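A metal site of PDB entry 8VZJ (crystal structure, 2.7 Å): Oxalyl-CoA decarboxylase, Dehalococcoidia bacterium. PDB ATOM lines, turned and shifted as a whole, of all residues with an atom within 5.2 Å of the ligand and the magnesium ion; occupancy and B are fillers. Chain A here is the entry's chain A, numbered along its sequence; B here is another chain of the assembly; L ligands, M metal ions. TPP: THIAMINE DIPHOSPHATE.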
ATOM      1  N   TYR A 370     -23.360  14.115 -15.737  1.00  0.00           N
ATOM      2  CA  TYR A 370     -22.411  15.178 -16.052  1.00  0.00           C
ATOM      3  C   TYR A 370     -23.091  16.542 -16.026  1.00  0.00           C
ATOM      4  O   TYR A 370     -22.484  17.535 -15.606  1.00  0.00           O
ATOM      5  CB  TYR A 370     -21.777  14.936 -17.417  1.00  0.00           C
ATOM      6  CG  TYR A 370     -20.763  13.817 -17.478  1.00  0.00           C
ATOM      7  CD1 TYR A 370     -19.424  14.054 -17.218  1.00  0.00           C
ATOM      8  CD2 TYR A 370     -21.153  12.526 -17.815  1.00  0.00           C
ATOM      9  CE1 TYR A 370     -18.493  13.036 -17.276  1.00  0.00           C
ATOM     10  CE2 TYR A 370     -20.232  11.499 -17.876  1.00  0.00           C
ATOM     11  CZ  TYR A 370     -18.902  11.754 -17.606  1.00  0.00           C
ATOM     12  OH  TYR A 370     -17.971  10.737 -17.665  1.00  0.00           O
ATOM     13  N   GLU A 390      -9.719  18.100 -18.346  1.00  0.00           N
ATOM     14  CA  GLU A 390      -9.056  16.950 -18.934  1.00  0.00           C
ATOM     15  C   GLU A 390      -9.877  15.697 -18.684  1.00  0.00           C
ATOM     16  O   GLU A 390     -10.369  15.479 -17.579  1.00  0.00           O
ATOM     17  CB  GLU A 390      -7.643  16.775 -18.366  1.00  0.00           C
ATOM     18  CG  GLU A 390      -6.808  15.730 -19.093  1.00  0.00           C
ATOM     19  CD  GLU A 390      -5.432  15.529 -18.466  1.00  0.00           C
ATOM     20  OE1 GLU A 390      -5.341  15.554 -17.218  1.00  0.00           O
ATOM     21  OE2 GLU A 390      -4.456  15.344 -19.222  1.00  0.00           O
ATOM     22  N   GLY A 391     -10.007  14.876 -19.716  1.00  0.00           N
ATOM     23  CA  GLY A 391     -10.753  13.639 -19.630  1.00  0.00           C
ATOM     24  C   GLY A 391     -11.362  13.291 -20.972  1.00  0.00           C
ATOM     25  O   GLY A 391     -10.943  13.817 -22.000  1.00  0.00           O
ATOM     26  N   ALA A 392     -12.331  12.386 -20.943  1.00  0.00           N
ATOM     27  CA  ALA A 392     -13.065  12.019 -22.152  1.00  0.00           C
ATOM     28  C   ALA A 392     -14.387  12.779 -22.206  1.00  0.00           C
ATOM     29  O   ALA A 392     -14.440  13.922 -22.663  1.00  0.00           O
ATOM     30  CB  ALA A 392     -13.305  10.513 -22.205  1.00  0.00           C
ATOM     31  N   SER A 393     -15.465  12.143 -21.736  1.00  0.00           N
ATOM     32  CA  SER A 393     -16.748  12.831 -21.655  1.00  0.00           C
ATOM     33  C   SER A 393     -16.662  14.030 -20.720  1.00  0.00           C
ATOM     34  O   SER A 393     -17.279  15.069 -20.983  1.00  0.00           O
ATOM     35  CB  SER A 393     -17.838  11.869 -21.191  1.00  0.00           C
ATOM     36  OG  SER A 393     -18.117  10.892 -22.177  1.00  0.00           O
ATOM     37  N   THR A 394     -15.898  13.903 -19.639  1.00  0.00           N
ATOM     38  CA  THR A 394     -15.720  15.024 -18.710  1.00  0.00           C
ATOM     39  C   THR A 394     -15.168  16.247 -19.426  1.00  0.00           C
ATOM     40  O   THR A 394     -15.593  17.375 -19.155  1.00  0.00           O
ATOM     41  CB  THR A 394     -14.790  14.607 -17.569  1.00  0.00           C
ATOM     42  OG1 THR A 394     -15.334  13.478 -16.889  1.00  0.00           O
ATOM     43  CG2 THR A 394     -14.609  15.754 -16.579  1.00  0.00           C
ATOM     44  N   MET A 395     -14.245  16.043 -20.367  1.00  0.00           N
ATOM     45  CA  MET A 395     -13.656  17.165 -21.095  1.00  0.00           C
ATOM     46  C   MET A 395     -14.574  17.657 -22.202  1.00  0.00           C
ATOM     47  O   MET A 395     -14.678  18.870 -22.437  1.00  0.00           O
ATOM     48  CB  MET A 395     -12.300  16.768 -21.666  1.00  0.00           C
ATOM     49  CG  MET A 395     -11.522  17.907 -22.301  1.00  0.00           C
ATOM     50  SD  MET A 395      -9.947  17.353 -22.968  1.00  0.00           S
ATOM     51  CE  MET A 395     -10.494  16.146 -24.176  1.00  0.00           C
ATOM     52  N   GLY A 417      -4.611  15.226 -27.878  1.00  0.00           N
ATOM     53  CA  GLY A 417      -5.515  14.418 -27.058  1.00  0.00           C
ATOM     54  C   GLY A 417      -4.828  13.772 -25.880  1.00  0.00           C
ATOM     55  O   GLY A 417      -5.110  12.604 -25.563  1.00  0.00           O
ATOM     56  N   THR A 418      -3.931  14.492 -25.217  1.00  0.00           N
ATOM     57  CA  THR A 418      -3.043  13.900 -24.234  1.00  0.00           C
ATOM     58  C   THR A 418      -3.713  13.782 -22.882  1.00  0.00           C
ATOM     59  O   THR A 418      -4.359  14.726 -22.409  1.00  0.00           O
ATOM     60  CB  THR A 418      -1.770  14.745 -24.103  1.00  0.00           C
ATOM     61  OG1 THR A 418      -1.218  14.995 -25.407  1.00  0.00           O
ATOM     62  CG2 THR A 418      -0.743  14.021 -23.252  1.00  0.00           C
ATOM     63  N   MET A 419      -3.560  12.620 -22.250  1.00  0.00           N
ATOM     64  CA  MET A 419      -3.895  12.440 -20.843  1.00  0.00           C
ATOM     65  C   MET A 419      -2.616  12.569 -20.023  1.00  0.00           C
ATOM     66  O   MET A 419      -1.592  11.981 -20.384  1.00  0.00           O
ATOM     67  CB  MET A 419      -4.569  11.091 -20.598  1.00  0.00           C
ATOM     68  CG  MET A 419      -5.981  10.978 -21.159  1.00  0.00           C
ATOM     69  SD  MET A 419      -7.115  12.203 -20.488  1.00  0.00           S
ATOM     70  CE  MET A 419      -7.257  13.335 -21.875  1.00  0.00           C
ATOM     71  N   GLY A 443     -11.356  14.014 -15.056  1.00  0.00           N
ATOM     72  CA  GLY A 443     -11.935  12.707 -14.899  1.00  0.00           C
ATOM     73  C   GLY A 443     -11.110  11.855 -13.958  1.00  0.00           C
ATOM     74  O   GLY A 443      -9.919  12.096 -13.749  1.00  0.00           O
ATOM     75  N   ASP A 444     -11.760  10.840 -13.368  1.00  0.00           N
ATOM     76  CA  ASP A 444     -11.047   9.992 -12.412  1.00  0.00           C
ATOM     77  C   ASP A 444      -9.877   9.265 -13.071  1.00  0.00           C
ATOM     78  O   ASP A 444      -8.865   9.012 -12.417  1.00  0.00           O
ATOM     79  CB  ASP A 444     -12.013   8.992 -11.767  1.00  0.00           C
ATOM     80  CG  ASP A 444     -12.795   8.193 -12.785  1.00  0.00           C
ATOM     81  OD1 ASP A 444     -13.252   8.790 -13.777  1.00  0.00           O
ATOM     82  OD2 ASP A 444     -12.963   6.978 -12.589  1.00  0.00           O
ATOM     83  N   SER A 445     -10.002   8.925 -14.354  1.00  0.00           N
ATOM     84  CA  SER A 445      -8.888   8.316 -15.071  1.00  0.00           C
ATOM     85  C   SER A 445      -7.791   9.334 -15.340  1.00  0.00           C
ATOM     86  O   SER A 445      -6.610   9.071 -15.107  1.00  0.00           O
ATOM     87  CB  SER A 445      -9.366   7.689 -16.375  1.00  0.00           C
ATOM     88  OG  SER A 445      -8.282   7.150 -17.120  1.00  0.00           O
ATOM     89  N   ALA A 446      -8.176  10.527 -15.824  1.00  0.00           N
ATOM     90  CA  ALA A 446      -7.193  11.554 -16.142  1.00  0.00           C
ATOM     91  C   ALA A 446      -6.432  12.011 -14.903  1.00  0.00           C
ATOM     92  O   ALA A 446      -5.247  12.341 -14.982  1.00  0.00           O
ATOM     93  CB  ALA A 446      -7.870  12.739 -16.823  1.00  0.00           C
ATOM     94  N   PHE A 449      -3.081  10.136 -13.888  1.00  0.00           N
ATOM     95  CA  PHE A 449      -1.859  10.291 -14.672  1.00  0.00           C
ATOM     96  C   PHE A 449      -0.834  11.166 -13.956  1.00  0.00           C
ATOM     97  O   PHE A 449       0.373  10.918 -14.070  1.00  0.00           O
ATOM     98  CB  PHE A 449      -2.173  10.878 -16.043  1.00  0.00           C
ATOM     99  CG  PHE A 449      -2.763   9.897 -17.005  1.00  0.00           C
ATOM    100  CD1 PHE A 449      -4.116   9.577 -16.956  1.00  0.00           C
ATOM    101  CD2 PHE A 449      -1.975   9.295 -17.971  1.00  0.00           C
ATOM    102  CE1 PHE A 449      -4.662   8.670 -17.840  1.00  0.00           C
ATOM    103  CE2 PHE A 449      -2.520   8.390 -18.869  1.00  0.00           C
ATOM    104  CZ  PHE A 449      -3.864   8.078 -18.804  1.00  0.00           C
ATOM    105  N   ILE A 470     -14.476  14.406 -11.436  1.00  0.00           N
ATOM    106  CA  ILE A 470     -15.763  13.849 -11.854  1.00  0.00           C
ATOM    107  C   ILE A 470     -15.538  12.349 -12.035  1.00  0.00           C
ATOM    108  O   ILE A 470     -14.956  11.915 -13.031  1.00  0.00           O
ATOM    109  CB  ILE A 470     -16.283  14.521 -13.118  1.00  0.00           C
ATOM    110  CG1 ILE A 470     -16.519  16.016 -12.854  1.00  0.00           C
ATOM    111  CG2 ILE A 470     -17.565  13.863 -13.581  1.00  0.00           C
ATOM    112  CD1 ILE A 470     -17.072  16.761 -14.044  1.00  0.00           C
ATOM    113  N   ASN A 472     -16.542   8.510 -12.473  1.00  0.00           N
ATOM    114  CA  ASN A 472     -17.482   7.501 -12.952  1.00  0.00           C
ATOM    115  C   ASN A 472     -16.913   6.088 -12.826  1.00  0.00           C
ATOM    116  O   ASN A 472     -17.393   5.168 -13.493  1.00  0.00           O
ATOM    117  CB  ASN A 472     -17.887   7.790 -14.395  1.00  0.00           C
ATOM    118  CG  ASN A 472     -16.705   7.800 -15.338  1.00  0.00           C
ATOM    119  OD1 ASN A 472     -15.549   7.810 -14.915  1.00  0.00           O
ATOM    120  ND2 ASN A 472     -16.992   7.802 -16.644  1.00  0.00           N
ATOM    121  N   ASN A 473     -15.889   5.910 -11.988  1.00  0.00           N
ATOM    122  CA  ASN A 473     -15.346   4.603 -11.634  1.00  0.00           C
ATOM    123  C   ASN A 473     -14.740   3.880 -12.835  1.00  0.00           C
ATOM    124  O   ASN A 473     -14.841   2.662 -12.965  1.00  0.00           O
ATOM    125  CB  ASN A 473     -16.409   3.717 -10.971  1.00  0.00           C
ATOM    126  CG  ASN A 473     -16.696   4.126  -9.538  1.00  0.00           C
ATOM    127  OD1 ASN A 473     -15.841   4.696  -8.857  1.00  0.00           O
ATOM    128  ND2 ASN A 473     -17.899   3.825  -9.062  1.00  0.00           N
ATOM    129  N   GLY A 474     -14.075   4.621 -13.709  1.00  0.00           N
ATOM    130  CA  GLY A 474     -13.356   3.994 -14.797  1.00  0.00           C
ATOM    131  C   GLY A 474     -13.150   4.923 -15.971  1.00  0.00           C
ATOM    132  O   GLY A 474     -13.499   6.101 -15.932  1.00  0.00           O
ATOM    133  N   ILE A 475     -12.575   4.350 -17.024  1.00  0.00           N
ATOM    134  CA  ILE A 475     -12.368   5.042 -18.290  1.00  0.00           C
ATOM    135  C   ILE A 475     -13.680   4.960 -19.063  1.00  0.00           C
ATOM    136  O   ILE A 475     -14.012   3.922 -19.638  1.00  0.00           O
ATOM    137  CB  ILE A 475     -11.202   4.435 -19.090  1.00  0.00           C
ATOM    138  CG1 ILE A 475      -9.900   4.533 -18.294  1.00  0.00           C
ATOM    139  CG2 ILE A 475     -11.079   5.112 -20.450  1.00  0.00           C
ATOM    140  CD1 ILE A 475      -8.694   3.998 -19.038  1.00  0.00           C
ATOM    141  N   GLY A 476     -14.434   6.052 -19.069  1.00  0.00           N
ATOM    142  CA  GLY A 476     -15.747   6.023 -19.690  1.00  0.00           C
ATOM    143  C   GLY A 476     -16.778   5.238 -18.917  1.00  0.00           C
ATOM    144  O   GLY A 476     -17.792   4.841 -19.496  1.00  0.00           O
ATOM    145  N   GLY A 477     -16.541   4.999 -17.635  1.00  0.00           N
ATOM    146  CA  GLY A 477     -17.475   4.247 -16.822  1.00  0.00           C
ATOM    147  C   GLY A 477     -16.897   2.954 -16.270  1.00  0.00           C
ATOM    148  O   GLY A 477     -15.890   2.459 -16.776  1.00  0.00           O
ATOM    149  N   ILE B  28      -2.603   1.261 -20.527  1.00  0.00           N
ATOM    150  CA  ILE B  28      -3.879   1.950 -20.388  1.00  0.00           C
ATOM    151  C   ILE B  28      -4.635   1.834 -21.711  1.00  0.00           C
ATOM    152  O   ILE B  28      -4.048   2.027 -22.786  1.00  0.00           O
ATOM    153  CB  ILE B  28      -3.684   3.425 -20.006  1.00  0.00           C
ATOM    154  CG1 ILE B  28      -2.890   3.526 -18.711  1.00  0.00           C
ATOM    155  CG2 ILE B  28      -5.032   4.114 -19.850  1.00  0.00           C
ATOM    156  CD1 ILE B  28      -2.553   4.925 -18.304  1.00  0.00           C
ATOM    157  N   VAL B  29      -5.920   1.506 -21.624  1.00  0.00           N
ATOM    158  CA  VAL B  29      -6.740   1.302 -22.807  1.00  0.00           C
ATOM    159  C   VAL B  29      -7.134   2.647 -23.405  1.00  0.00           C
ATOM    160  O   VAL B  29      -6.994   3.692 -22.768  1.00  0.00           O
ATOM    161  CB  VAL B  29      -7.991   0.464 -22.492  1.00  0.00           C
ATOM    162  CG1 VAL B  29      -7.584  -0.880 -21.915  1.00  0.00           C
ATOM    163  CG2 VAL B  29      -8.897   1.217 -21.526  1.00  0.00           C
ATOM    164  N   GLY B  30      -7.640   2.617 -24.629  1.00  0.00           N
ATOM    165  CA  GLY B  30      -8.015   3.826 -25.339  1.00  0.00           C
ATOM    166  C   GLY B  30      -7.938   3.596 -26.829  1.00  0.00           C
ATOM    167  O   GLY B  30      -7.557   2.529 -27.301  1.00  0.00           O
ATOM    168  N   ILE B  31      -8.303   4.652 -27.561  1.00  0.00           N
ATOM    169  CA  ILE B  31      -8.292   4.564 -29.027  1.00  0.00           C
ATOM    170  C   ILE B  31      -6.863   4.363 -29.507  1.00  0.00           C
ATOM    171  O   ILE B  31      -5.963   5.138 -29.122  1.00  0.00           O
ATOM    172  CB  ILE B  31      -8.905   5.843 -29.641  1.00  0.00           C
ATOM    173  CG1 ILE B  31     -10.322   6.064 -29.114  1.00  0.00           C
ATOM    174  CG2 ILE B  31      -8.901   5.754 -31.165  1.00  0.00           C
ATOM    175  CD1 ILE B  31     -11.294   4.975 -29.500  1.00  0.00           C
ATOM    176  N   GLU B  53       1.235   5.247 -18.448  1.00  0.00           N
ATOM    177  CA  GLU B  53       2.000   4.325 -19.290  1.00  0.00           C
ATOM    178  C   GLU B  53       3.470   4.274 -18.900  1.00  0.00           C
ATOM    179  O   GLU B  53       4.141   3.281 -19.178  1.00  0.00           O
ATOM    180  CB  GLU B  53       1.881   4.719 -20.764  1.00  0.00           C
ATOM    181  CG  GLU B  53       0.544   4.382 -21.404  1.00  0.00           C
ATOM    182  CD  GLU B  53      -0.402   5.554 -21.395  1.00  0.00           C
ATOM    183  OE1 GLU B  53      -0.133   6.546 -20.673  1.00  0.00           O
ATOM    184  OE2 GLU B  53      -1.416   5.499 -22.131  1.00  0.00           O
ATOM    185  N   VAL B  76      -1.852   3.728 -26.209  1.00  0.00           N
ATOM    186  CA  VAL B  76      -2.647   4.293 -27.298  1.00  0.00           C
ATOM    187  C   VAL B  76      -1.734   5.027 -28.265  1.00  0.00           C
ATOM    188  O   VAL B  76      -0.518   5.111 -28.049  1.00  0.00           O
ATOM    189  CB  VAL B  76      -3.736   5.243 -26.765  1.00  0.00           C
ATOM    190  CG1 VAL B  76      -4.573   4.545 -25.709  1.00  0.00           C
ATOM    191  CG2 VAL B  76      -3.115   6.509 -26.203  1.00  0.00           C
ATOM    192  N   PRO B  79       0.450  10.201 -27.578  1.00  0.00           N
ATOM    193  CA  PRO B  79       0.911  10.394 -26.190  1.00  0.00           C
ATOM    194  C   PRO B  79       1.074   9.104 -25.404  1.00  0.00           C
ATOM    195  O   PRO B  79       2.021   8.970 -24.629  1.00  0.00           O
ATOM    196  CB  PRO B  79      -0.181  11.280 -25.587  1.00  0.00           C
ATOM    197  CG  PRO B  79      -0.774  11.998 -26.742  1.00  0.00           C
ATOM    198  CD  PRO B  79      -0.710  11.055 -27.909  1.00  0.00           C
ATOM    199  N   GLY B  80       0.157   8.143 -25.581  1.00  0.00           N
ATOM    200  CA  GLY B  80       0.256   6.906 -24.821  1.00  0.00           C
ATOM    201  C   GLY B  80       1.511   6.117 -25.127  1.00  0.00           C
ATOM    202  O   GLY B  80       2.188   5.636 -24.219  1.00  0.00           O
ATOM    203  N   HIS B  83       4.800   7.921 -23.806  1.00  0.00           N
ATOM    204  CA  HIS B  83       5.025   7.685 -22.381  1.00  0.00           C
ATOM    205  C   HIS B  83       5.698   6.345 -22.137  1.00  0.00           C
ATOM    206  O   HIS B  83       6.457   6.196 -21.168  1.00  0.00           O
ATOM    207  CB  HIS B  83       3.716   7.765 -21.603  1.00  0.00           C
ATOM    208  CG  HIS B  83       3.097   9.117 -21.584  1.00  0.00           C
ATOM    209  ND1 HIS B  83       1.884   9.370 -20.968  1.00  0.00           N
ATOM    210  CD2 HIS B  83       3.514  10.306 -22.091  1.00  0.00           C
ATOM    211  CE1 HIS B  83       1.584  10.650 -21.105  1.00  0.00           C
ATOM    212  NE2 HIS B  83       2.557  11.234 -21.775  1.00  0.00           N
ATOM    213  N   PHE B 115      -5.880  11.843 -35.534  1.00  0.00           N
ATOM    214  CA  PHE B 115      -5.879  11.889 -34.080  1.00  0.00           C
ATOM    215  C   PHE B 115      -4.641  11.171 -33.546  1.00  0.00           C
ATOM    216  O   PHE B 115      -4.444   9.982 -33.803  1.00  0.00           O
ATOM    217  CB  PHE B 115      -7.154  11.240 -33.538  1.00  0.00           C
ATOM    218  CG  PHE B 115      -7.284  11.324 -32.037  1.00  0.00           C
ATOM    219  CD1 PHE B 115      -7.423  12.548 -31.405  1.00  0.00           C
ATOM    220  CD2 PHE B 115      -7.277  10.165 -31.270  1.00  0.00           C
ATOM    221  CE1 PHE B 115      -7.540  12.613 -30.028  1.00  0.00           C
ATOM    222  CE2 PHE B 115      -7.406  10.234 -29.900  1.00  0.00           C
ATOM    223  CZ  PHE B 115      -7.532  11.456 -29.275  1.00  0.00           C
ATOM    224  N   GLN B 116      -3.818  11.910 -32.799  1.00  0.00           N
ATOM    225  CA  GLN B 116      -2.612  11.371 -32.153  1.00  0.00           C
ATOM    226  C   GLN B 116      -1.630  10.805 -33.187  1.00  0.00           C
ATOM    227  O   GLN B 116      -0.914   9.844 -32.907  1.00  0.00           O
ATOM    228  CB  GLN B 116      -2.968  10.327 -31.098  1.00  0.00           C
ATOM    229  CG  GLN B 116      -3.871  10.878 -30.004  1.00  0.00           C
ATOM    230  CD  GLN B 116      -4.253   9.852 -28.955  1.00  0.00           C
ATOM    231  OE1 GLN B 116      -4.332   8.653 -29.231  1.00  0.00           O
ATOM    232  NE2 GLN B 116      -4.501  10.317 -27.734  1.00  0.00           N
HETATM  233  N1' TPP L   1      -3.086   7.711 -22.434  1.00  0.00           N
HETATM  234  C2' TPP L   1      -2.795   8.907 -22.970  1.00  0.00           C
HETATM  235  CM2 TPP L   1      -1.431   9.454 -22.705  1.00  0.00           C
HETATM  236  N3' TPP L   1      -3.617   9.648 -23.712  1.00  0.00           N
HETATM  237  C4' TPP L   1      -4.850   9.166 -23.959  1.00  0.00           C
HETATM  238  N4' TPP L   1      -5.668   9.924 -24.698  1.00  0.00           N
HETATM  239  C5' TPP L   1      -5.252   7.896 -23.449  1.00  0.00           C
HETATM  240  C6' TPP L   1      -4.308   7.240 -22.693  1.00  0.00           C
HETATM  241  C7' TPP L   1      -6.620   7.315 -23.683  1.00  0.00           C
HETATM  242  N3  TPP L   1      -7.696   8.087 -23.025  1.00  0.00           N
HETATM  243  C2  TPP L   1      -8.437   8.988 -23.638  1.00  0.00           C
HETATM  244  S1  TPP L   1      -9.553   9.704 -22.619  1.00  0.00           S
HETATM  245  C5  TPP L   1      -8.998   8.756 -21.286  1.00  0.00           C
HETATM  246  C4  TPP L   1      -7.990   7.936 -21.669  1.00  0.00           C
HETATM  247  CM4 TPP L   1      -7.241   6.967 -20.829  1.00  0.00           C
HETATM  248  C6  TPP L   1      -9.602   8.890 -19.914  1.00  0.00           C
HETATM  249  C7  TPP L   1     -11.103   8.711 -19.917  1.00  0.00           C
HETATM  250  O7  TPP L   1     -11.556   8.615 -18.541  1.00  0.00           O
HETATM  251  PA  TPP L   1     -11.889   9.865 -17.631  1.00  0.00           P
HETATM  252  O1A TPP L   1     -10.768  10.824 -17.599  1.00  0.00           O
HETATM  253  O2A TPP L   1     -12.318   9.340 -16.260  1.00  0.00           O
HETATM  254  O3A TPP L   1     -13.177  10.482 -18.327  1.00  0.00           O
HETATM  255  PB  TPP L   1     -14.735  10.219 -18.432  1.00  0.00           P
HETATM  256  O1B TPP L   1     -15.027   9.024 -19.272  1.00  0.00           O
HETATM  257  O2B TPP L   1     -15.194  10.069 -16.979  1.00  0.00           O
HETATM  258  O3B TPP L   1     -15.307  11.519 -19.005  1.00  0.00           O
HETATM  259 MG    MG M   1     -14.003   8.314 -16.064  1.00  0.00          MG
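Residues that only touch the ligand: Gly 391 (3.5 Å), Gly 443 (3.5 Å), Gly 80 of chain B (3.5 Å), His 83 of chain B (3.6 Å), Pro 79 of chain B (3.6 Å), Ile 475 (3.6 Å), Phe 449 (3.7 Å), Ile 28 of chain B (3.7 Å), Val 76 of chain B (3.8 Å) and Val 29 of chain B (3.8 Å).
Within 4 Å of the ligand: Tyr 370, Gly 391, Ala 392, Ser 393, Thr 394, Gly 417, Met 419, Gly 443, Asp 444, Ser 445, Ala 446, Phe 449, Asn 472, Gly 474, Ile 475, Gly 476, Ile 28 of chain B, Val 29 of chain B, Glu 53 of chain B, Val 76 of chain B, Pro 79 of chain B, Gly 80 of chain B, His 83 of chain B and Gln 116 of chain B.
OE1 of Glu 53 of chain B lies within hydrogen-bond range of ND1 of His 83 of chain B (3.5 Å).
The backbone NH (N) of Asn 473 is in hydrogen-bond range of the side-chain carboxylate (OD2) of Asp 444.
NE2 of Gln 116 of chain B sits at hydrogen-bond distance from O of Gly 417 (3.2 Å).
The side-chain amide nitrogen (ND2) of Asn 472 lies close to the backbone NH (N) of Gly 477 (3.0 Å).
The side-chain amide nitrogen (ND2) of Asn 472 sits at hydrogen-bond distance from the side-chain hydroxyl (OH) of Tyr 370 (3.3 Å).
N of Gly 443 is in hydrogen-bond range of O of Glu 390 (3.1 Å).
O of Ile 470 sits at hydrogen-bond distance from N of Asp 444, 3.4 Å away.
Merely in contact with the magnesium ion: Gly 476 (3.8 Å).
The magnesium ion is bound by O2A of the ligand (2.0 Å), OD1 of Asn 472 (2.0 Å), O of Gly 474 (2.3 Å), O2B of the ligand (2.3 Å) and OD1 of Asp 444 (2.5 Å).
The backbone NH of Thr 394 is in hydrogen-bond range of an oxygen (O3B) of the ligand, 2.5 Å away.
A nitrogen (N1') of the ligand is in hydrogen-bond range of the side-chain carboxylate of Glu 53 of chain B.
The side-chain hydroxyl (OG1) of Thr 394 lies within hydrogen-bond range of an oxygen (O3B) of the ligand.
The backbone NH of Ser 445 lies close to an oxygen (O2A) of the ligand (3.0 Å).
An oxygen (O1B) of the ligand lies within hydrogen-bond range of the backbone NH (N) of Gly 476, 3.0 Å away.
N of Ala 392 is in hydrogen-bond range of O3A of the ligand, 3.3 Å away.
The side-chain hydroxyl of Tyr 370 lies within hydrogen-bond range of an oxygen (O3B) of the ligand, 3.1 Å away.
N of Ala 446 is in hydrogen-bond range of O1A of the ligand.
O2A of the ligand lies close to N of Asp 444.
N4' of the ligand lies within hydrogen-bond range of O of Gly 417 (2.9 Å).
The backbone NH (N) of Ser 393 sits at hydrogen-bond distance from an oxygen (O3B) of the ligand (2.8 Å).
The side-chain amide nitrogen (NE2) of Gln 116 of chain B lies close to a nitrogen (N4') of the ligand, at 3.3 Å.
A nitrogen (N3') of the ligand lies within hydrogen-bond range of the backbone NH of Met 419 (3.3 Å).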
